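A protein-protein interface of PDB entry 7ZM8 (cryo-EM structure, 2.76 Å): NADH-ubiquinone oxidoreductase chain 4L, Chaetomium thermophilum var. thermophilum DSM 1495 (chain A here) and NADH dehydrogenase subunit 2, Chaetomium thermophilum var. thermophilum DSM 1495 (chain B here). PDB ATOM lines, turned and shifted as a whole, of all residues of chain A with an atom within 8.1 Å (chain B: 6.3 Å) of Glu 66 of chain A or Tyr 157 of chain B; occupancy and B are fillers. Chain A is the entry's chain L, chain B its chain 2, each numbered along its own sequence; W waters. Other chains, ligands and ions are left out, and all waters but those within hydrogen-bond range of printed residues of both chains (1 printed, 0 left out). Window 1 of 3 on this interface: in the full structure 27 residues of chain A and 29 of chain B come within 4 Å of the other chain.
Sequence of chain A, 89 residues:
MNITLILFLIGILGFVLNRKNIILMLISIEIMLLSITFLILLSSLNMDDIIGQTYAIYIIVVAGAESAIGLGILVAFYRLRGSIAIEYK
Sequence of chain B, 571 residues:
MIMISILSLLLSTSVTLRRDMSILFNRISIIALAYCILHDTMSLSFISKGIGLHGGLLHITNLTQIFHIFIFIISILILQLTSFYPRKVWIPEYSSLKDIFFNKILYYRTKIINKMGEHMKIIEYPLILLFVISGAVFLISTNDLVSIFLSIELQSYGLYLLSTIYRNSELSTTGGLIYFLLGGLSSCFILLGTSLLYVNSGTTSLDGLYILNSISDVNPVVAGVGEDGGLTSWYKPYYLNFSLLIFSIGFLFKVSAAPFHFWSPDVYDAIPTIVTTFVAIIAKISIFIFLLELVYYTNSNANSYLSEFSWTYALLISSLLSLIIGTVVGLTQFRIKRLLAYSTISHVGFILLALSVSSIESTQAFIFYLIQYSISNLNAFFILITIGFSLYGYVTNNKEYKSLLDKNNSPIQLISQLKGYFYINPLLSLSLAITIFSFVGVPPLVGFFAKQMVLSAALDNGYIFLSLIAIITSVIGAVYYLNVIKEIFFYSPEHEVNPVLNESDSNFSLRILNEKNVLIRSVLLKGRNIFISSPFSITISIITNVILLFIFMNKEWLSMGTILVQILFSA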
ATOM      1  N   MET A  25      25.014   7.327   0.412  1.00  0.00           N
ATOM      2  CA  MET A  25      23.852   7.906   1.083  1.00  0.00           C
ATOM      3  C   MET A  25      23.696   7.373   2.500  1.00  0.00           C
ATOM      4  O   MET A  25      23.200   8.081   3.378  1.00  0.00           O
ATOM      5  CB  MET A  25      22.559   7.682   0.299  1.00  0.00           C
ATOM      6  CG  MET A  25      22.471   8.404  -1.019  1.00  0.00           C
ATOM      7  SD  MET A  25      20.868   8.113  -1.775  1.00  0.00           S
ATOM      8  CE  MET A  25      21.078   6.436  -2.308  1.00  0.00           C
ATOM      9  N   LEU A  26      24.093   6.123   2.742  1.00  0.00           N
ATOM     10  CA  LEU A  26      24.184   5.650   4.119  1.00  0.00           C
ATOM     11  C   LEU A  26      25.216   6.442   4.901  1.00  0.00           C
ATOM     12  O   LEU A  26      24.998   6.779   6.069  1.00  0.00           O
ATOM     13  CB  LEU A  26      24.531   4.164   4.158  1.00  0.00           C
ATOM     14  CG  LEU A  26      23.387   3.160   4.069  1.00  0.00           C
ATOM     15  CD1 LEU A  26      22.498   3.331   5.279  1.00  0.00           C
ATOM     16  CD2 LEU A  26      22.599   3.303   2.802  1.00  0.00           C
ATOM     17  N   ILE A  29      23.993  10.132   5.682  1.00  0.00           N
ATOM     18  CA  ILE A  29      22.979  10.188   6.771  1.00  0.00           C
ATOM     19  C   ILE A  29      23.691  10.198   8.123  1.00  0.00           C
ATOM     20  O   ILE A  29      23.295  10.993   8.985  1.00  0.00           O
ATOM     21  CB  ILE A  29      21.970   9.027   6.639  1.00  0.00           C
ATOM     22  CG1 ILE A  29      20.952   9.282   5.524  1.00  0.00           C
ATOM     23  CG2 ILE A  29      21.275   8.743   7.961  1.00  0.00           C
ATOM     24  CD1 ILE A  29      20.051   8.105   5.243  1.00  0.00           C
ATOM     25  N   GLU A  30      24.722   9.382   8.282  1.00  0.00           N
ATOM     26  CA  GLU A  30      25.503   9.300   9.535  1.00  0.00           C
ATOM     27  C   GLU A  30      26.300  10.580   9.816  1.00  0.00           C
ATOM     28  O   GLU A  30      26.375  10.968  10.981  1.00  0.00           O
ATOM     29  CB  GLU A  30      26.359   8.041   9.473  1.00  0.00           C
ATOM     30  CG  GLU A  30      25.587   6.794   9.849  1.00  0.00           C
ATOM     31  CD  GLU A  30      26.421   5.761  10.583  1.00  0.00           C
ATOM     32  OE1 GLU A  30      27.300   5.154   9.942  1.00  0.00           O
ATOM     33  OE2 GLU A  30      26.198   5.578  11.797  1.00  0.00           O
ATOM     34  N   LEU A  33      23.814  12.953  11.253  1.00  0.00           N
ATOM     35  CA  LEU A  33      23.514  12.595  12.663  1.00  0.00           C
ATOM     36  C   LEU A  33      24.649  13.050  13.578  1.00  0.00           C
ATOM     37  O   LEU A  33      24.331  13.574  14.643  1.00  0.00           O
ATOM     38  CB  LEU A  33      23.261  11.090  12.747  1.00  0.00           C
ATOM     39  CG  LEU A  33      22.068  10.585  11.939  1.00  0.00           C
ATOM     40  CD1 LEU A  33      22.020   9.067  11.916  1.00  0.00           C
ATOM     41  CD2 LEU A  33      20.766  11.159  12.465  1.00  0.00           C
ATOM     42  N   ILE A  59      20.633   9.397  20.687  1.00  0.00           N
ATOM     43  CA  ILE A  59      20.731   9.607  19.218  1.00  0.00           C
ATOM     44  C   ILE A  59      21.784   8.651  18.669  1.00  0.00           C
ATOM     45  O   ILE A  59      21.568   8.141  17.579  1.00  0.00           O
ATOM     46  CB  ILE A  59      21.056  11.081  18.906  1.00  0.00           C
ATOM     47  CG1 ILE A  59      19.883  12.014  19.200  1.00  0.00           C
ATOM     48  CG2 ILE A  59      21.538  11.252  17.474  1.00  0.00           C
ATOM     49  CD1 ILE A  59      20.264  13.463  19.101  1.00  0.00           C
ATOM     50  N   ILE A  60      22.817   8.345  19.443  1.00  0.00           N
ATOM     51  CA  ILE A  60      23.876   7.377  19.037  1.00  0.00           C
ATOM     52  C   ILE A  60      23.291   5.965  18.966  1.00  0.00           C
ATOM     53  O   ILE A  60      23.659   5.229  18.056  1.00  0.00           O
ATOM     54  CB  ILE A  60      25.083   7.497  19.988  1.00  0.00           C
ATOM     55  CG1 ILE A  60      25.761   8.865  19.874  1.00  0.00           C
ATOM     56  CG2 ILE A  60      26.077   6.366  19.786  1.00  0.00           C
ATOM     57  CD1 ILE A  60      26.719   9.165  21.001  1.00  0.00           C
ATOM     58  N   VAL A  61      22.413   5.609  19.898  1.00  0.00           N
ATOM     59  CA  VAL A  61      21.788   4.258  19.946  1.00  0.00           C
ATOM     60  C   VAL A  61      20.854   4.098  18.748  1.00  0.00           C
ATOM     61  O   VAL A  61      20.943   3.071  18.083  1.00  0.00           O
ATOM     62  CB  VAL A  61      21.037   4.079  21.281  1.00  0.00           C
ATOM     63  CG1 VAL A  61      20.244   2.788  21.343  1.00  0.00           C
ATOM     64  CG2 VAL A  61      21.963   4.199  22.477  1.00  0.00           C
ATOM     65  N   VAL A  62      19.957   5.051  18.536  1.00  0.00           N
ATOM     66  CA  VAL A  62      19.030   5.035  17.373  1.00  0.00           C
ATOM     67  C   VAL A  62      19.842   5.076  16.074  1.00  0.00           C
ATOM     68  O   VAL A  62      19.450   4.423  15.107  1.00  0.00           O
ATOM     69  CB  VAL A  62      17.981   6.160  17.480  1.00  0.00           C
ATOM     70  CG1 VAL A  62      17.306   6.468  16.156  1.00  0.00           C
ATOM     71  CG2 VAL A  62      16.952   5.870  18.555  1.00  0.00           C
ATOM     72  N   ALA A  63      20.932   5.822  16.056  1.00  0.00           N
ATOM     73  CA  ALA A  63      21.761   5.906  14.847  1.00  0.00           C
ATOM     74  C   ALA A  63      22.355   4.540  14.509  1.00  0.00           C
ATOM     75  O   ALA A  63      22.338   4.186  13.322  1.00  0.00           O
ATOM     76  CB  ALA A  63      22.818   6.952  15.051  1.00  0.00           C
ATOM     77  N   GLY A  64      22.882   3.819  15.498  1.00  0.00           N
ATOM     78  CA  GLY A  64      23.403   2.464  15.273  1.00  0.00           C
ATOM     79  C   GLY A  64      22.291   1.531  14.863  1.00  0.00           C
ATOM     80  O   GLY A  64      22.522   0.704  13.986  1.00  0.00           O
ATOM     81  N   ALA A  65      21.126   1.646  15.485  1.00  0.00           N
ATOM     82  CA  ALA A  65      19.980   0.767  15.167  1.00  0.00           C
ATOM     83  C   ALA A  65      19.558   0.982  13.717  1.00  0.00           C
ATOM     84  O   ALA A  65      19.233   0.004  13.059  1.00  0.00           O
ATOM     85  CB  ALA A  65      18.857   1.028  16.129  1.00  0.00           C
ATOM     86  N   GLU A  66      19.554   2.217  13.218  1.00  0.00           N
ATOM     87  CA  GLU A  66      19.221   2.412  11.781  1.00  0.00           C
ATOM     88  C   GLU A  66      20.326   1.840  10.900  1.00  0.00           C
ATOM     89  O   GLU A  66      20.005   1.362   9.812  1.00  0.00           O
ATOM     90  CB  GLU A  66      18.915   3.865  11.421  1.00  0.00           C
ATOM     91  CG  GLU A  66      20.097   4.802  11.358  1.00  0.00           C
ATOM     92  CD  GLU A  66      19.662   6.240  11.151  1.00  0.00           C
ATOM     93  OE1 GLU A  66      19.360   6.916  12.154  1.00  0.00           O
ATOM     94  OE2 GLU A  66      19.596   6.669   9.985  1.00  0.00           O
ATOM     95  N   SER A  67      21.575   1.910  11.353  1.00  0.00           N
ATOM     96  CA  SER A  67      22.680   1.312  10.580  1.00  0.00           C
ATOM     97  C   SER A  67      22.463  -0.190  10.451  1.00  0.00           C
ATOM     98  O   SER A  67      22.641  -0.715   9.350  1.00  0.00           O
ATOM     99  CB  SER A  67      23.935   1.600  11.301  1.00  0.00           C
ATOM    100  OG  SER A  67      24.078   2.995  11.517  1.00  0.00           O
ATOM    101  N   ALA A  68      22.067  -0.843  11.531  1.00  0.00           N
ATOM    102  CA  ALA A  68      21.773  -2.285  11.495  1.00  0.00           C
ATOM    103  C   ALA A  68      20.582  -2.568  10.587  1.00  0.00           C
ATOM    104  O   ALA A  68      20.680  -3.484   9.769  1.00  0.00           O
ATOM    105  CB  ALA A  68      21.437  -2.708  12.903  1.00  0.00           C
ATOM    106  N   ILE A  69      19.504  -1.804  10.742  1.00  0.00           N
ATOM    107  CA  ILE A  69      18.267  -2.026   9.943  1.00  0.00           C
ATOM    108  C   ILE A  69      18.578  -1.738   8.471  1.00  0.00           C
ATOM    109  O   ILE A  69      18.084  -2.467   7.623  1.00  0.00           O
ATOM    110  CB  ILE A  69      17.103  -1.203  10.537  1.00  0.00           C
ATOM    111  CG1 ILE A  69      16.584  -1.834  11.829  1.00  0.00           C
ATOM    112  CG2 ILE A  69      15.977  -1.011   9.531  1.00  0.00           C
ATOM    113  CD1 ILE A  69      16.195  -3.278  11.669  1.00  0.00           C
ATOM    114  N   GLY A  70      19.353  -0.692   8.196  1.00  0.00           N
ATOM    115  CA  GLY A  70      19.729  -0.326   6.827  1.00  0.00           C
ATOM    116  C   GLY A  70      20.653  -1.293   6.136  1.00  0.00           C
ATOM    117  O   GLY A  70      20.450  -1.510   4.940  1.00  0.00           O
ATOM    118  N   LEU A  71      21.669  -1.797   6.839  1.00  0.00           N
ATOM    119  CA  LEU A  71      22.658  -2.667   6.171  1.00  0.00           C
ATOM    120  C   LEU A  71      22.033  -4.047   6.061  1.00  0.00           C
ATOM    121  O   LEU A  71      22.430  -4.785   5.165  1.00  0.00           O
ATOM    122  CB  LEU A  71      23.987  -2.651   6.924  1.00  0.00           C
ATOM    123  CG  LEU A  71      24.849  -1.407   6.721  1.00  0.00           C
ATOM    124  CD1 LEU A  71      26.094  -1.467   7.589  1.00  0.00           C
ATOM    125  CD2 LEU A  71      25.227  -1.243   5.260  1.00  0.00           C
ATOM    126  N   GLY A  72      21.065  -4.353   6.923  1.00  0.00           N
ATOM    127  CA  GLY A  72      20.345  -5.596   6.725  1.00  0.00           C
ATOM    128  C   GLY A  72      19.459  -5.573   5.497  1.00  0.00           C
ATOM    129  O   GLY A  72      19.374  -6.562   4.765  1.00  0.00           O
ATOM    130  N   ILE A  73      18.773  -4.454   5.265  1.00  0.00           N
ATOM    131  CA  ILE A  73      17.943  -4.323   4.074  1.00  0.00           C
ATOM    132  C   ILE A  73      18.814  -4.303   2.827  1.00  0.00           C
ATOM    133  O   ILE A  73      18.442  -4.842   1.780  1.00  0.00           O
ATOM    134  CB  ILE A  73      17.056  -3.068   4.179  1.00  0.00           C
ATOM    135  CG1 ILE A  73      15.982  -3.268   5.243  1.00  0.00           C
ATOM    136  CG2 ILE A  73      16.397  -2.740   2.853  1.00  0.00           C
ATOM    137  CD1 ILE A  73      15.116  -2.060   5.473  1.00  0.00           C
ATOM    138  N   ILE B 128       5.686  -7.595  14.194  1.00  0.00           N
ATOM    139  CA  ILE B 128       6.262  -6.346  13.712  1.00  0.00           C
ATOM    140  C   ILE B 128       5.193  -5.276  13.538  1.00  0.00           C
ATOM    141  O   ILE B 128       5.472  -4.088  13.720  1.00  0.00           O
ATOM    142  CB  ILE B 128       7.057  -6.605  12.420  1.00  0.00           C
ATOM    143  CG1 ILE B 128       8.177  -7.601  12.708  1.00  0.00           C
ATOM    144  CG2 ILE B 128       7.661  -5.324  11.886  1.00  0.00           C
ATOM    145  CD1 ILE B 128       9.213  -7.700  11.627  1.00  0.00           C
ATOM    146  N   VAL B 132       5.127  -1.455  15.133  1.00  0.00           N
ATOM    147  CA  VAL B 132       4.728  -0.223  14.462  1.00  0.00           C
ATOM    148  C   VAL B 132       3.613   0.461  15.234  1.00  0.00           C
ATOM    149  O   VAL B 132       3.641   1.677  15.445  1.00  0.00           O
ATOM    150  CB  VAL B 132       4.312  -0.507  13.008  1.00  0.00           C
ATOM    151  CG1 VAL B 132       3.937   0.784  12.309  1.00  0.00           C
ATOM    152  CG2 VAL B 132       5.416  -1.209  12.262  1.00  0.00           C
ATOM    153  N   PHE B 149      11.241  12.052  18.935  1.00  0.00           N
ATOM    154  CA  PHE B 149      12.227  11.464  18.043  1.00  0.00           C
ATOM    155  C   PHE B 149      12.290   9.955  18.206  1.00  0.00           C
ATOM    156  O   PHE B 149      12.339   9.218  17.216  1.00  0.00           O
ATOM    157  CB  PHE B 149      13.598  12.081  18.296  1.00  0.00           C
ATOM    158  CG  PHE B 149      14.690  11.439  17.505  1.00  0.00           C
ATOM    159  CD1 PHE B 149      14.774  11.638  16.141  1.00  0.00           C
ATOM    160  CD2 PHE B 149      15.612  10.617  18.116  1.00  0.00           C
ATOM    161  CE1 PHE B 149      15.760  11.034  15.410  1.00  0.00           C
ATOM    162  CE2 PHE B 149      16.598  10.017  17.389  1.00  0.00           C
ATOM    163  CZ  PHE B 149      16.675  10.227  16.037  1.00  0.00           C
ATOM    164  N   ILE B 152       9.037   8.378  16.705  1.00  0.00           N
ATOM    165  CA  ILE B 152       8.888   8.445  15.225  1.00  0.00           C
ATOM    166  C   ILE B 152       9.773   7.374  14.603  1.00  0.00           C
ATOM    167  O   ILE B 152       9.306   6.716  13.672  1.00  0.00           O
ATOM    168  CB  ILE B 152       9.081   9.868  14.637  1.00  0.00           C
ATOM    169  CG1 ILE B 152       8.538   9.967  13.211  1.00  0.00           C
ATOM    170  CG2 ILE B 152      10.520  10.349  14.722  1.00  0.00           C
ATOM    171  CD1 ILE B 152       7.102   9.526  13.072  1.00  0.00           C
ATOM    172  N   GLU B 153      10.988   7.209  15.115  1.00  0.00           N
ATOM    173  CA  GLU B 153      11.911   6.150  14.636  1.00  0.00           C
ATOM    174  C   GLU B 153      11.355   4.757  14.938  1.00  0.00           C
ATOM    175  O   GLU B 153      11.409   3.920  14.048  1.00  0.00           O
ATOM    176  CB  GLU B 153      13.305   6.358  15.230  1.00  0.00           C
ATOM    177  CG  GLU B 153      13.898   7.716  14.902  1.00  0.00           C
ATOM    178  CD  GLU B 153      14.022   8.056  13.425  1.00  0.00           C
ATOM    179  OE1 GLU B 153      15.011   7.627  12.803  1.00  0.00           O
ATOM    180  OE2 GLU B 153      13.135   8.758  12.902  1.00  0.00           O
ATOM    181  N   LEU B 154      10.804   4.535  16.127  1.00  0.00           N
ATOM    182  CA  LEU B 154      10.159   3.234  16.422  1.00  0.00           C
ATOM    183  C   LEU B 154       9.110   2.917  15.349  1.00  0.00           C
ATOM    184  O   LEU B 154       9.048   1.757  14.922  1.00  0.00           O
ATOM    185  CB  LEU B 154       9.530   3.262  17.814  1.00  0.00           C
ATOM    186  CG  LEU B 154       9.082   1.919  18.382  1.00  0.00           C
ATOM    187  CD1 LEU B 154      10.114   0.834  18.116  1.00  0.00           C
ATOM    188  CD2 LEU B 154       8.815   2.040  19.871  1.00  0.00           C
ATOM    189  N   GLN B 155       8.325   3.914  14.923  1.00  0.00           N
ATOM    190  CA  GLN B 155       7.334   3.642  13.889  1.00  0.00           C
ATOM    191  C   GLN B 155       7.986   3.475  12.525  1.00  0.00           C
ATOM    192  O   GLN B 155       7.613   2.581  11.758  1.00  0.00           O
ATOM    193  CB  GLN B 155       6.305   4.765  13.857  1.00  0.00           C
ATOM    194  CG  GLN B 155       5.257   4.607  12.789  1.00  0.00           C
ATOM    195  CD  GLN B 155       4.238   5.708  12.812  1.00  0.00           C
ATOM    196  OE1 GLN B 155       3.052   5.460  12.981  1.00  0.00           O
ATOM    197  NE2 GLN B 155       4.692   6.939  12.638  1.00  0.00           N
ATOM    198  N   SER B 156       8.864   4.392  12.151  1.00  0.00           N
ATOM    199  CA  SER B 156       9.538   4.371  10.824  1.00  0.00           C
ATOM    200  C   SER B 156      10.327   3.085  10.589  1.00  0.00           C
ATOM    201  O   SER B 156      10.201   2.534   9.511  1.00  0.00           O
ATOM    202  CB  SER B 156      10.420   5.573  10.700  1.00  0.00           C
ATOM    203  OG  SER B 156       9.663   6.772  10.720  1.00  0.00           O
ATOM    204  N   TYR B 157      11.140   2.664  11.548  1.00  0.00           N
ATOM    205  CA  TYR B 157      12.011   1.474  11.404  1.00  0.00           C
ATOM    206  C   TYR B 157      11.188   0.203  11.220  1.00  0.00           C
ATOM    207  O   TYR B 157      11.665  -0.710  10.553  1.00  0.00           O
ATOM    208  CB  TYR B 157      13.032   1.370  12.542  1.00  0.00           C
ATOM    209  CG  TYR B 157      14.050   2.474  12.635  1.00  0.00           C
ATOM    210  CD1 TYR B 157      14.390   3.236  11.533  1.00  0.00           C
ATOM    211  CD2 TYR B 157      14.685   2.744  13.833  1.00  0.00           C
ATOM    212  CE1 TYR B 157      15.327   4.250  11.624  1.00  0.00           C
ATOM    213  CE2 TYR B 157      15.629   3.749  13.941  1.00  0.00           C
ATOM    214  CZ  TYR B 157      15.951   4.505  12.831  1.00  0.00           C
ATOM    215  OH  TYR B 157      16.875   5.500  12.926  1.00  0.00           O
ATOM    216  N   GLY B 158      10.000   0.158  11.800  1.00  0.00           N
ATOM    217  CA  GLY B 158       9.165  -1.044  11.688  1.00  0.00           C
ATOM    218  C   GLY B 158       8.458  -1.046  10.357  1.00  0.00           C
ATOM    219  O   GLY B 158       8.239  -2.135   9.834  1.00  0.00           O
ATOM    220  N   LEU B 159       8.110   0.123   9.832  1.00  0.00           N
ATOM    221  CA  LEU B 159       7.556   0.235   8.490  1.00  0.00           C
ATOM    222  C   LEU B 159       8.568  -0.187   7.432  1.00  0.00           C
ATOM    223  O   LEU B 159       8.195  -0.794   6.424  1.00  0.00           O
ATOM    224  CB  LEU B 159       7.064   1.658   8.248  1.00  0.00           C
ATOM    225  CG  LEU B 159       5.732   1.964   8.936  1.00  0.00           C
ATOM    226  CD1 LEU B 159       5.416   3.442   8.910  1.00  0.00           C
ATOM    227  CD2 LEU B 159       4.612   1.169   8.308  1.00  0.00           C
ATOM    228  N   TYR B 160       9.852   0.123   7.642  1.00  0.00           N
ATOM    229  CA  TYR B 160      10.883  -0.331   6.712  1.00  0.00           C
ATOM    230  C   TYR B 160      10.981  -1.847   6.704  1.00  0.00           C
ATOM    231  O   TYR B 160      11.149  -2.462   5.648  1.00  0.00           O
ATOM    232  CB  TYR B 160      12.246   0.265   7.070  1.00  0.00           C
ATOM    233  CG  TYR B 160      12.293   1.767   7.169  1.00  0.00           C
ATOM    234  CD1 TYR B 160      11.384   2.559   6.488  1.00  0.00           C
ATOM    235  CD2 TYR B 160      13.251   2.390   7.950  1.00  0.00           C
ATOM    236  CE1 TYR B 160      11.425   3.923   6.588  1.00  0.00           C
ATOM    237  CE2 TYR B 160      13.300   3.753   8.051  1.00  0.00           C
ATOM    238  CZ  TYR B 160      12.383   4.512   7.368  1.00  0.00           C
ATOM    239  OH  TYR B 160      12.427   5.872   7.473  1.00  0.00           O
ATOM    240  N   LEU B 161      10.889  -2.462   7.879  1.00  0.00           N
ATOM    241  CA  LEU B 161      10.999  -3.909   7.990  1.00  0.00           C
ATOM    242  C   LEU B 161       9.786  -4.614   7.409  1.00  0.00           C
ATOM    243  O   LEU B 161       9.905  -5.730   6.899  1.00  0.00           O
ATOM    244  CB  LEU B 161      11.182  -4.293   9.451  1.00  0.00           C
ATOM    245  CG  LEU B 161      12.514  -3.845  10.034  1.00  0.00           C
ATOM    246  CD1 LEU B 161      12.473  -3.929  11.546  1.00  0.00           C
ATOM    247  CD2 LEU B 161      13.641  -4.683   9.461  1.00  0.00           C
ATOM    248  N   LEU B 162       8.611  -3.997   7.512  1.00  0.00           N
ATOM    249  CA  LEU B 162       7.420  -4.542   6.877  1.00  0.00           C
ATOM    250  C   LEU B 162       7.571  -4.569   5.368  1.00  0.00           C
ATOM    251  O   LEU B 162       7.168  -5.532   4.710  1.00  0.00           O
ATOM    252  CB  LEU B 162       6.209  -3.708   7.265  1.00  0.00           C
ATOM    253  CG  LEU B 162       5.669  -3.890   8.668  1.00  0.00           C
ATOM    254  CD1 LEU B 162       4.324  -3.234   8.732  1.00  0.00           C
ATOM    255  CD2 LEU B 162       5.552  -5.373   8.975  1.00  0.00           C
ATOM    256  N   PHE B 180      13.702   3.028   3.353  1.00  0.00           N
ATOM    257  CA  PHE B 180      14.694   3.267   4.427  1.00  0.00           C
ATOM    258  C   PHE B 180      15.607   4.421   4.068  1.00  0.00           C
ATOM    259  O   PHE B 180      15.953   5.209   4.945  1.00  0.00           O
ATOM    260  CB  PHE B 180      15.582   2.043   4.652  1.00  0.00           C
ATOM    261  CG  PHE B 180      16.815   2.326   5.467  1.00  0.00           C
ATOM    262  CD1 PHE B 180      16.758   2.341   6.848  1.00  0.00           C
ATOM    263  CD2 PHE B 180      18.023   2.611   4.851  1.00  0.00           C
ATOM    264  CE1 PHE B 180      17.884   2.636   7.595  1.00  0.00           C
ATOM    265  CE2 PHE B 180      19.143   2.923   5.600  1.00  0.00           C
ATOM    266  CZ  PHE B 180      19.072   2.933   6.970  1.00  0.00           C
ATOM    267  N   GLY B 184      15.294   7.798   6.047  1.00  0.00           N
ATOM    268  CA  GLY B 184      16.412   8.249   6.896  1.00  0.00           C
ATOM    269  C   GLY B 184      16.778   9.697   6.677  1.00  0.00           C
ATOM    270  O   GLY B 184      17.147  10.369   7.638  1.00  0.00           O
ATOM    271  N   SER B 187      14.390  11.557   8.588  1.00  0.00           N
ATOM    272  CA  SER B 187      14.639  11.528  10.022  1.00  0.00           C
ATOM    273  C   SER B 187      15.676  12.561  10.440  1.00  0.00           C
ATOM    274  O   SER B 187      15.602  13.094  11.550  1.00  0.00           O
ATOM    275  CB  SER B 187      15.082  10.130  10.437  1.00  0.00           C
ATOM    276  OG  SER B 187      14.154   9.159   9.989  1.00  0.00           O
ATOM    277  N   CYS B 188      16.644  12.852   9.573  1.00  0.00           N
ATOM    278  CA  CYS B 188      17.611  13.904   9.857  1.00  0.00           C
ATOM    279  C   CYS B 188      16.931  15.259  10.003  1.00  0.00           C
ATOM    280  O   CYS B 188      17.297  16.053  10.874  1.00  0.00           O
ATOM    281  CB  CYS B 188      18.666  13.955   8.753  1.00  0.00           C
ATOM    282  SG  CYS B 188      20.019  12.769   8.924  1.00  0.00           S
HETATM  283  O   HOH W   1      18.248   9.404   9.899  1.00  0.00           O
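Water W1 lies within hydrogen-bond range of the backbone carbonyl oxygen of Gly 184 of chain B and the side-chain carboxylate of Glu 66 of chain A.
Hydrophobic or aromatic side chains of chain A that line the printed part of chain B: Leu 26, Ile 29, Leu 33, Val 62, Ile 69 and Ile 73.
Printed residues of chain B that touch a printed residue of chain A: Phe 149, Glu 153, Tyr 157, Tyr 160, Leu 161, Phe 180, Gly 184 and Cys 188.
Hydrophobic or aromatic side chains of chain B that line the printed part of chain A: Phe 149, Tyr 157, Leu 161 and Phe 180.
Along chain B the printed residues that touch a printed residue of chain A span positions 149 to 188.
Among the printed residues, 12 pairs touch across the chains.
Among the printed residues, no Asp or Glu carboxylate lies within 4 Å of a Lys or Arg side-chain nitrogen of the other chain.
O of Ile 29 of chain A is in hydrogen-bond range of SG of Cys 188 of chain B.
OE1 of Glu 66 of chain A lies within hydrogen-bond range of OH of Tyr 157 of chain B (3.0 Å).
Among the printed residues, merely in contact across the chains: Leu 26 of chain A with Phe 180 of chain B, Ile 29 of chain A with Gly 184 of chain B, Leu 33 of chain A with Cys 188 of chain B, Val 62 of chain A with Phe 149 of chain B, Val 62 of chain A with Glu 153 of chain B, Val 62 of chain A with Tyr 157 of chain B, Glu 66 of chain A with Phe 180 of chain B, Ile 69 of chain A with Leu 161 of chain B, Gly 70 of chain A with Phe 180 of chain B and Ile 73 of chain A with Tyr 160 of chain B.
Ile 60 of chain A touches none of the printed residues of chain B.
Glu 66 of chain A touches just these residues of chain B: Tyr 157 and Phe 180.
Of the printed residues of chain B, Gly 70 of chain A touches Phe 180 (3.3 Å).
Tyr 157 of chain B touches just these residues of chain A: Val 62 and Glu 66.
Of the printed residues of chain A, Cys 188 of chain B touches Ile 29 (3.7 Å) and Leu 33 (3.96 Å).
The nearest printed residue of chain B that does not touch Leu 26 of chain A is Gly 184 of chain B (8.0 Å).
OE2 of Glu 153 of chain B sits at hydrogen-bond distance from OG of Ser 187 of chain B, at 3.1 Å.
The side-chain hydroxyl of Tyr 157 of chain B sits at hydrogen-bond distance from the side-chain carboxylate of Glu 153 of chain B (2.8 Å).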
